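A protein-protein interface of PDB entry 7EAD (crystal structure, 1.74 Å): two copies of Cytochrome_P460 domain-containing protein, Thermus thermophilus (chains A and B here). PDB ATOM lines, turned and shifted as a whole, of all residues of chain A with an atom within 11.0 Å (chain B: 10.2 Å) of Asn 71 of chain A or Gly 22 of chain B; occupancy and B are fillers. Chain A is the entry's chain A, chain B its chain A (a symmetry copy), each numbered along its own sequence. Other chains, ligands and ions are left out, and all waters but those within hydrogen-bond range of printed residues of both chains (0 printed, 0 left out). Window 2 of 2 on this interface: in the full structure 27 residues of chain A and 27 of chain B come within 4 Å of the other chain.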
ATOM      1  N   LYS A  20     -11.264 -17.655 -25.071  1.00  0.00           N
ATOM      2  CA  LYS A  20     -12.237 -18.487 -24.394  1.00  0.00           C
ATOM      3  C   LYS A  20     -11.621 -19.680 -23.650  1.00  0.00           C
ATOM      4  O   LYS A  20     -10.526 -20.067 -23.951  1.00  0.00           O
ATOM      5  CB  LYS A  20     -13.229 -19.008 -25.429  1.00  0.00           C
ATOM      6  CG  LYS A  20     -14.014 -17.982 -26.217  1.00  0.00           C
ATOM      7  CD  LYS A  20     -14.791 -18.665 -27.331  1.00  0.00           C
ATOM      8  CE  LYS A  20     -15.498 -17.724 -28.278  1.00  0.00           C
ATOM      9  NZ  LYS A  20     -16.497 -17.008 -27.495  1.00  0.00           N
ATOM     10  N   LYS A  67     -18.391 -11.286 -20.470  1.00  0.00           N
ATOM     11  CA  LYS A  67     -19.673 -11.644 -19.878  1.00  0.00           C
ATOM     12  C   LYS A  67     -20.626 -12.059 -20.990  1.00  0.00           C
ATOM     13  O   LYS A  67     -20.853 -11.293 -21.929  1.00  0.00           O
ATOM     14  CB  LYS A  67     -20.249 -10.463 -19.105  1.00  0.00           C
ATOM     15  CG  LYS A  67     -19.720 -10.296 -17.695  1.00  0.00           C
ATOM     16  CD  LYS A  67     -19.976  -8.869 -17.208  1.00  0.00           C
ATOM     17  CE  LYS A  67     -21.456  -8.557 -17.026  1.00  0.00           C
ATOM     18  NZ  LYS A  67     -21.677  -7.087 -16.873  1.00  0.00           N
ATOM     19  N   VAL A  68     -21.191 -13.257 -20.887  1.00  0.00           N
ATOM     20  CA  VAL A  68     -22.184 -13.721 -21.849  1.00  0.00           C
ATOM     21  C   VAL A  68     -23.555 -13.620 -21.196  1.00  0.00           C
ATOM     22  O   VAL A  68     -23.838 -14.326 -20.225  1.00  0.00           O
ATOM     23  CB  VAL A  68     -21.896 -15.149 -22.320  1.00  0.00           C
ATOM     24  CG1 VAL A  68     -23.088 -15.682 -23.105  1.00  0.00           C
ATOM     25  CG2 VAL A  68     -20.643 -15.171 -23.176  1.00  0.00           C
ATOM     26  N   GLU A  69     -24.404 -12.741 -21.726  1.00  0.00           N
ATOM     27  CA  GLU A  69     -25.762 -12.546 -21.231  1.00  0.00           C
ATOM     28  C   GLU A  69     -26.692 -12.334 -22.416  1.00  0.00           C
ATOM     29  O   GLU A  69     -26.416 -11.488 -23.272  1.00  0.00           O
ATOM     30  CB  GLU A  69     -25.868 -11.321 -20.305  1.00  0.00           C
ATOM     31  CG  GLU A  69     -24.662 -11.022 -19.439  1.00  0.00           C
ATOM     32  CD  GLU A  69     -24.764 -11.618 -18.047  1.00  0.00           C
ATOM     33  OE1 GLU A  69     -25.631 -12.496 -17.828  1.00  0.00           O
ATOM     34  OE2 GLU A  69     -23.965 -11.209 -17.172  1.00  0.00           O
ATOM     35  N   GLY A  70     -27.800 -13.073 -22.458  1.00  0.00           N
ATOM     36  CA  GLY A  70     -28.873 -12.765 -23.395  1.00  0.00           C
ATOM     37  C   GLY A  70     -28.460 -12.605 -24.850  1.00  0.00           C
ATOM     38  O   GLY A  70     -28.786 -11.597 -25.493  1.00  0.00           O
ATOM     39  N   ASN A  71     -27.743 -13.603 -25.369  1.00  0.00           N
ATOM     40  CA  ASN A  71     -27.270 -13.629 -26.755  1.00  0.00           C
ATOM     41  C   ASN A  71     -26.355 -12.446 -27.054  1.00  0.00           C
ATOM     42  O   ASN A  71     -26.410 -11.852 -28.130  1.00  0.00           O
ATOM     43  CB  ASN A  71     -28.434 -13.682 -27.744  1.00  0.00           C
ATOM     44  CG  ASN A  71     -29.265 -14.952 -27.591  1.00  0.00           C
ATOM     45  OD1 ASN A  71     -28.724 -16.046 -27.427  1.00  0.00           O
ATOM     46  ND2 ASN A  71     -30.574 -14.808 -27.648  1.00  0.00           N
ATOM     47  N   ALA A  72     -25.507 -12.101 -26.093  1.00  0.00           N
ATOM     48  CA  ALA A  72     -24.541 -11.032 -26.305  1.00  0.00           C
ATOM     49  C   ALA A  72     -23.277 -11.329 -25.510  1.00  0.00           C
ATOM     50  O   ALA A  72     -23.326 -11.947 -24.444  1.00  0.00           O
ATOM     51  CB  ALA A  72     -25.109  -9.657 -25.910  1.00  0.00           C
ATOM     52  N   LEU A  73     -22.138 -10.894 -26.048  1.00  0.00           N
ATOM     53  CA  LEU A  73     -20.903 -10.820 -25.282  1.00  0.00           C
ATOM     54  C   LEU A  73     -20.751  -9.380 -24.812  1.00  0.00           C
ATOM     55  O   LEU A  73     -20.695  -8.465 -25.637  1.00  0.00           O
ATOM     56  CB  LEU A  73     -19.687 -11.242 -26.110  1.00  0.00           C
ATOM     57  CG  LEU A  73     -18.373 -11.153 -25.333  1.00  0.00           C
ATOM     58  CD1 LEU A  73     -18.384 -12.119 -24.164  1.00  0.00           C
ATOM     59  CD2 LEU A  73     -17.177 -11.414 -26.245  1.00  0.00           C
ATOM     60  N   LEU A  74     -20.695  -9.185 -23.497  1.00  0.00           N
ATOM     61  CA  LEU A  74     -20.589  -7.868 -22.887  1.00  0.00           C
ATOM     62  C   LEU A  74     -19.217  -7.693 -22.251  1.00  0.00           C
ATOM     63  O   LEU A  74     -18.605  -8.652 -21.777  1.00  0.00           O
ATOM     64  CB  LEU A  74     -21.664  -7.651 -21.810  1.00  0.00           C
ATOM     65  CG  LEU A  74     -23.106  -7.376 -22.238  1.00  0.00           C
ATOM     66  CD1 LEU A  74     -23.715  -8.597 -22.844  1.00  0.00           C
ATOM     67  CD2 LEU A  74     -23.922  -6.943 -21.029  1.00  0.00           C
ATOM     68  N   GLU A  75     -18.743  -6.454 -22.236  1.00  0.00           N
ATOM     69  CA  GLU A  75     -17.519  -6.147 -21.516  1.00  0.00           C
ATOM     70  C   GLU A  75     -17.767  -6.216 -20.015  1.00  0.00           C
ATOM     71  O   GLU A  75     -18.640  -5.522 -19.485  1.00  0.00           O
ATOM     72  CB  GLU A  75     -16.997  -4.776 -21.936  1.00  0.00           C
ATOM     73  CG  GLU A  75     -16.652  -4.727 -23.430  1.00  0.00           C
ATOM     74  CD  GLU A  75     -16.239  -3.344 -23.906  1.00  0.00           C
ATOM     75  OE1 GLU A  75     -17.044  -2.393 -23.759  1.00  0.00           O
ATOM     76  OE2 GLU A  75     -15.110  -3.222 -24.430  1.00  0.00           O
ATOM     77  N   MET B  17     -19.179  -4.771 -28.134  1.00  0.00           N
ATOM     78  CA  MET B  17     -20.221  -5.712 -27.804  1.00  0.00           C
ATOM     79  C   MET B  17     -20.482  -6.675 -28.949  1.00  0.00           C
ATOM     80  O   MET B  17     -20.450  -6.280 -30.040  1.00  0.00           O
ATOM     81  CB  MET B  17     -21.505  -4.959 -27.488  1.00  0.00           C
ATOM     82  CG  MET B  17     -22.616  -5.765 -26.876  1.00  0.00           C
ATOM     83  SD  MET B  17     -24.142  -4.794 -26.688  1.00  0.00           S
ATOM     84  CE  MET B  17     -25.065  -5.857 -25.656  1.00  0.00           C
ATOM     85  N   GLU B  18     -20.649  -7.959 -28.664  1.00  0.00           N
ATOM     86  CA  GLU B  18     -21.009  -8.941 -29.678  1.00  0.00           C
ATOM     87  C   GLU B  18     -22.485  -9.273 -29.534  1.00  0.00           C
ATOM     88  O   GLU B  18     -22.949  -9.565 -28.434  1.00  0.00           O
ATOM     89  CB  GLU B  18     -20.186 -10.229 -29.562  1.00  0.00           C
ATOM     90  CG  GLU B  18     -20.286 -11.100 -30.813  1.00  0.00           C
ATOM     91  CD  GLU B  18     -20.192 -12.599 -30.532  1.00  0.00           C
ATOM     92  OE1 GLU B  18     -19.906 -12.995 -29.382  1.00  0.00           O
ATOM     93  OE2 GLU B  18     -20.403 -13.384 -31.482  1.00  0.00           O
ATOM     94  N   LEU B  19     -23.213  -9.206 -30.641  1.00  0.00           N
ATOM     95  CA  LEU B  19     -24.596  -9.656 -30.705  1.00  0.00           C
ATOM     96  C   LEU B  19     -24.572 -11.019 -31.375  1.00  0.00           C
ATOM     97  O   LEU B  19     -24.074 -11.151 -32.498  1.00  0.00           O
ATOM     98  CB  LEU B  19     -25.475  -8.663 -31.473  1.00  0.00           C
ATOM     99  CG  LEU B  19     -25.484  -7.247 -30.869  1.00  0.00           C
ATOM    100  CD1 LEU B  19     -26.384  -6.263 -31.640  1.00  0.00           C
ATOM    101  CD2 LEU B  19     -25.887  -7.298 -29.402  1.00  0.00           C
ATOM    102  N   LYS B  20     -25.022 -12.017 -30.649  1.00  0.00           N
ATOM    103  CA  LYS B  20     -25.059 -13.401 -31.075  1.00  0.00           C
ATOM    104  C   LYS B  20     -26.419 -13.841 -31.635  1.00  0.00           C
ATOM    105  O   LYS B  20     -27.404 -13.215 -31.360  1.00  0.00           O
ATOM    106  CB  LYS B  20     -24.706 -14.282 -29.882  1.00  0.00           C
ATOM    107  CG  LYS B  20     -23.356 -14.067 -29.234  1.00  0.00           C
ATOM    108  CD  LYS B  20     -23.258 -14.877 -27.952  1.00  0.00           C
ATOM    109  CE  LYS B  20     -22.009 -14.628 -27.139  1.00  0.00           C
ATOM    110  NZ  LYS B  20     -20.882 -15.063 -27.953  1.00  0.00           N
ATOM    111  N   PRO B  21     -26.439 -14.910 -32.425  1.00  0.00           N
ATOM    112  CA  PRO B  21     -27.716 -15.427 -32.938  1.00  0.00           C
ATOM    113  C   PRO B  21     -28.776 -15.551 -31.849  1.00  0.00           C
ATOM    114  O   PRO B  21     -28.507 -15.997 -30.732  1.00  0.00           O
ATOM    115  CB  PRO B  21     -27.329 -16.795 -33.506  1.00  0.00           C
ATOM    116  CG  PRO B  21     -25.910 -16.595 -33.955  1.00  0.00           C
ATOM    117  CD  PRO B  21     -25.287 -15.681 -32.932  1.00  0.00           C
ATOM    118  N   GLY B  22     -30.000 -15.150 -32.188  1.00  0.00           N
ATOM    119  CA  GLY B  22     -31.092 -15.100 -31.255  1.00  0.00           C
ATOM    120  C   GLY B  22     -31.344 -13.714 -30.697  1.00  0.00           C
ATOM    121  O   GLY B  22     -32.475 -13.404 -30.303  1.00  0.00           O
ATOM    122  N   HIS B  23     -30.318 -12.876 -30.654  1.00  0.00           N
ATOM    123  CA  HIS B  23     -30.506 -11.508 -30.202  1.00  0.00           C
ATOM    124  C   HIS B  23     -31.527 -10.805 -31.091  1.00  0.00           C
ATOM    125  O   HIS B  23     -31.523 -11.000 -32.313  1.00  0.00           O
ATOM    126  CB  HIS B  23     -29.176 -10.757 -30.241  1.00  0.00           C
ATOM    127  CG  HIS B  23     -29.172  -9.503 -29.431  1.00  0.00           C
ATOM    128  ND1 HIS B  23     -29.625  -8.299 -29.923  1.00  0.00           N
ATOM    129  CD2 HIS B  23     -28.778  -9.268 -28.158  1.00  0.00           C
ATOM    130  CE1 HIS B  23     -29.504  -7.373 -28.988  1.00  0.00           C
ATOM    131  NE2 HIS B  23     -28.991  -7.934 -27.909  1.00  0.00           N
ATOM    132  N   PRO B  24     -32.417  -9.987 -30.521  1.00  0.00           N
ATOM    133  CA  PRO B  24     -33.405  -9.291 -31.364  1.00  0.00           C
ATOM    134  C   PRO B  24     -32.774  -8.415 -32.431  1.00  0.00           C
ATOM    135  O   PRO B  24     -33.415  -8.151 -33.456  1.00  0.00           O
ATOM    136  CB  PRO B  24     -34.226  -8.462 -30.360  1.00  0.00           C
ATOM    137  CG  PRO B  24     -33.411  -8.402 -29.118  1.00  0.00           C
ATOM    138  CD  PRO B  24     -32.552  -9.653 -29.094  1.00  0.00           C
ATOM    139  N   LEU B  25     -31.536  -7.966 -32.233  1.00  0.00           N
ATOM    140  CA  LEU B  25     -30.829  -7.146 -33.204  1.00  0.00           C
ATOM    141  C   LEU B  25     -29.838  -7.954 -34.040  1.00  0.00           C
ATOM    142  O   LEU B  25     -29.035  -7.365 -34.771  1.00  0.00           O
ATOM    143  CB  LEU B  25     -30.102  -5.993 -32.494  1.00  0.00           C
ATOM    144  CG  LEU B  25     -30.966  -4.983 -31.721  1.00  0.00           C
ATOM    145  CD1 LEU B  25     -30.112  -3.859 -31.150  1.00  0.00           C
ATOM    146  CD2 LEU B  25     -32.028  -4.415 -32.617  1.00  0.00           C
ATOM    147  N   TYR B  26     -29.887  -9.286 -33.968  1.00  0.00           N
ATOM    148  CA  TYR B  26     -28.901 -10.078 -34.698  1.00  0.00           C
ATOM    149  C   TYR B  26     -29.060  -9.922 -36.205  1.00  0.00           C
ATOM    150  O   TYR B  26     -28.064  -9.810 -36.930  1.00  0.00           O
ATOM    151  CB  TYR B  26     -28.988 -11.554 -34.315  1.00  0.00           C
ATOM    152  CG  TYR B  26     -27.888 -12.333 -34.987  1.00  0.00           C
ATOM    153  CD1 TYR B  26     -26.579 -12.210 -34.553  1.00  0.00           C
ATOM    154  CD2 TYR B  26     -28.143 -13.136 -36.090  1.00  0.00           C
ATOM    155  CE1 TYR B  26     -25.552 -12.893 -35.172  1.00  0.00           C
ATOM    156  CE2 TYR B  26     -27.116 -13.826 -36.721  1.00  0.00           C
ATOM    157  CZ  TYR B  26     -25.824 -13.694 -36.251  1.00  0.00           C
ATOM    158  OH  TYR B  26     -24.785 -14.368 -36.860  1.00  0.00           O
ATOM    159  N   GLU B  27     -30.299  -9.906 -36.706  1.00  0.00           N
ATOM    160  CA  GLU B  27     -30.476  -9.846 -38.156  1.00  0.00           C
ATOM    161  C   GLU B  27     -29.967  -8.533 -38.732  1.00  0.00           C
ATOM    162  O   GLU B  27     -29.417  -8.507 -39.841  1.00  0.00           O
ATOM    163  CB  GLU B  27     -31.943 -10.055 -38.526  1.00  0.00           C
ATOM    164  CG  GLU B  27     -32.190 -10.162 -40.029  1.00  0.00           C
ATOM    165  CD  GLU B  27     -33.660 -10.398 -40.365  1.00  0.00           C
ATOM    166  OE1 GLU B  27     -34.460  -9.428 -40.296  1.00  0.00           O
ATOM    167  OE2 GLU B  27     -34.014 -11.559 -40.679  1.00  0.00           O
ATOM    168  N   SER B  28     -30.135  -7.428 -37.999  1.00  0.00           N
ATOM    169  CA  SER B  28     -29.670  -6.140 -38.506  1.00  0.00           C
ATOM    170  C   SER B  28     -28.225  -5.836 -38.133  1.00  0.00           C
ATOM    171  O   SER B  28     -27.469  -5.335 -38.975  1.00  0.00           O
ATOM    172  CB  SER B  28     -30.574  -5.011 -38.004  1.00  0.00           C
ATOM    173  OG  SER B  28     -30.926  -5.221 -36.651  1.00  0.00           O
ATOM    174  N   PHE B  29     -27.815  -6.117 -36.891  1.00  0.00           N
ATOM    175  CA  PHE B  29     -26.487  -5.730 -36.422  1.00  0.00           C
ATOM    176  C   PHE B  29     -25.712  -6.893 -35.810  1.00  0.00           C
ATOM    177  O   PHE B  29     -24.853  -6.674 -34.951  1.00  0.00           O
ATOM    178  CB  PHE B  29     -26.574  -4.596 -35.405  1.00  0.00           C
ATOM    179  CG  PHE B  29     -27.291  -3.386 -35.905  1.00  0.00           C
ATOM    180  CD1 PHE B  29     -26.660  -2.498 -36.757  1.00  0.00           C
ATOM    181  CD2 PHE B  29     -28.592  -3.125 -35.505  1.00  0.00           C
ATOM    182  CE1 PHE B  29     -27.311  -1.366 -37.214  1.00  0.00           C
ATOM    183  CE2 PHE B  29     -29.250  -1.998 -35.964  1.00  0.00           C
ATOM    184  CZ  PHE B  29     -28.602  -1.117 -36.817  1.00  0.00           C
ATOM    185  N   GLY B  30     -25.994  -8.127 -36.227  1.00  0.00           N
ATOM    186  CA  GLY B  30     -25.298  -9.264 -35.644  1.00  0.00           C
ATOM    187  C   GLY B  30     -23.808  -9.217 -35.943  1.00  0.00           C
ATOM    188  O   GLY B  30     -23.383  -8.840 -37.037  1.00  0.00           O
ATOM    189  N   GLY B  31     -23.008  -9.609 -34.954  1.00  0.00           N
ATOM    190  CA  GLY B  31     -21.566  -9.629 -35.068  1.00  0.00           C
ATOM    191  C   GLY B  31     -20.937  -8.878 -33.921  1.00  0.00           C
ATOM    192  O   GLY B  31     -21.584  -8.564 -32.917  1.00  0.00           O
ATOM    193  N   LEU B  32     -19.644  -8.587 -34.062  1.00  0.00           N
ATOM    194  CA  LEU B  32     -18.902  -7.827 -33.068  1.00  0.00           C
ATOM    195  C   LEU B  32     -18.847  -6.381 -33.529  1.00  0.00           C
ATOM    196  O   LEU B  32     -18.393  -6.101 -34.647  1.00  0.00           O
ATOM    197  CB  LEU B  32     -17.483  -8.379 -32.886  1.00  0.00           C
ATOM    198  CG  LEU B  32     -16.554  -7.618 -31.932  1.00  0.00           C
ATOM    199  CD1 LEU B  32     -17.043  -7.622 -30.490  1.00  0.00           C
ATOM    200  CD2 LEU B  32     -15.150  -8.208 -32.001  1.00  0.00           C
ATOM    201  N   HIS B  33     -19.307  -5.464 -32.679  1.00  0.00           N
ATOM    202  CA  HIS B  33     -19.251  -4.059 -33.030  1.00  0.00           C
ATOM    203  C   HIS B  33     -18.457  -3.254 -32.006  1.00  0.00           C
ATOM    204  O   HIS B  33     -18.405  -3.579 -30.815  1.00  0.00           O
ATOM    205  CB  HIS B  33     -20.663  -3.458 -33.242  1.00  0.00           C
ATOM    206  CG  HIS B  33     -21.463  -3.257 -31.987  1.00  0.00           C
ATOM    207  ND1 HIS B  33     -22.467  -4.118 -31.598  1.00  0.00           N
ATOM    208  CD2 HIS B  33     -21.446  -2.261 -31.068  1.00  0.00           C
ATOM    209  CE1 HIS B  33     -23.022  -3.674 -30.482  1.00  0.00           C
ATOM    210  NE2 HIS B  33     -22.415  -2.550 -30.136  1.00  0.00           N
ATOM    211  N   ALA B  66     -18.190 -11.787 -36.542  1.00  0.00           N
ATOM    212  CA  ALA B  66     -17.629 -12.417 -35.360  1.00  0.00           C
ATOM    213  C   ALA B  66     -17.251 -13.838 -35.745  1.00  0.00           C
ATOM    214  O   ALA B  66     -18.126 -14.649 -36.074  1.00  0.00           O
ATOM    215  CB  ALA B  66     -18.633 -12.403 -34.206  1.00  0.00           C
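1 position is printed for both chains.
O of Met 17 of chain B lies within hydrogen-bond range of N of His 33 of chain B, at 3.0 Å.
NZ of Lys 20 of chain B lies within salt-bridge range of OE1 of Glu 18 of chain B, 2.7 Å away.
The backbone NH (N) of Leu 19 of chain B sits at hydrogen-bond distance from the backbone carbonyl oxygen (O) of Gly 31 of chain B, 2.9 Å away.
A ring nitrogen (ND1) of His 23 of chain B is in hydrogen-bond range of the backbone NH (N) of Leu 25 of chain B.
N of Lys 20 of chain B is in hydrogen-bond range of O of Asn 71 of chain A (2.9 Å).
The side-chain amide oxygen (OD1) of Asn 71 of chain A lies close to the backbone carbonyl oxygen (O) of Pro 21 of chain B (3.3 Å).
The backbone NH (N) of Leu 73 of chain A sits at hydrogen-bond distance from the backbone carbonyl oxygen (O) of Glu 18 of chain B (2.8 Å).
Of chain B, only Leu 19 (3.8 Å), Lys 20 (2.9 Å), Pro 21 (3.3 Å), Gly 22 (3.3 Å) and His 23 (3.5 Å) come within 4 Å of Asn 71 of chain A.
Of chain A, only Asn 71 comes within 4 Å of Gly 22 of chain B.
Of the printed residues of chain B, Gly 70 of chain A touches His 23.
Of chain B, only Met 17 (3.8 Å), Glu 18 (3.0 Å) and Lys 20 (3.9 Å) come within 4 Å of Ala 72 of chain A.
Lys 20 of chain B touches just these residues of chain A: Asn 71 (2.9 Å), Ala 72 (3.9 Å) and Leu 73 (3.9 Å).
Pro 21 of chain B touches just one residue of chain A: Asn 71 (3.3 Å).
His 23 of chain B touches just these residues of chain A: Gly 70 and Asn 71.
Pro 24 of chain B touches none of the printed residues of chain A.
Printed residues of chain A within 4 Å of Glu 18 of chain B: Ala 72 and Leu 73.
Of the printed residues of chain B, Leu 73 of chain A touches Met 17, Glu 18 and Lys 20.
Printed residues of chain A within 4 Å of Met 17 of chain B: Ala 72 (3.8 Å) and Leu 73 (3.5 Å).
Leu 74 of chain A touches none of the printed residues of chain B.
The nearest residue of chain A that does not touch Gly 22 of chain B is Gly 70 of chain A (6.2 Å).
Hydrophobic or aromatic side chains of chain A that line the printed part of chain B: Ala 72 and Leu 73.
Of the 18 printed residues of chain B, 7 touch a printed residue of chain A.
Printed residues of chain B that touch a printed residue of chain A: Met 17, Glu 18, Leu 19, Lys 20, Pro 21, Gly 22 and His 23.
Hydrophobic or aromatic side chains of chain B that line the printed part of chain A: Met 17 and His 23.
Among the printed residues, no Asp or Glu carboxylate lies within 4 Å of a Lys or Arg side-chain nitrogen of the other chain.
Gly 70 of chain A touches His 23 of chain B.
Leu 19 of chain B touches Asn 71 of chain A (C to O, 3.8 Å).
ND2 of Asn 71 of chain A touches C of Gly 22 of chain B, at 3.3 Å.
His 23 of chain B touches Asn 71 of chain A.
CB of Ala 72 of chain A touches CE of Met 17 of chain B (3.8 Å).
Ala 72 of chain A touches Glu 18 of chain B.
Ala 72 of chain A touches Lys 20 of chain B.
Leu 73 of chain A touches Met 17 of chain B.
N of Leu 73 of chain A touches CE of Lys 20 of chain B, 3.9 Å away.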
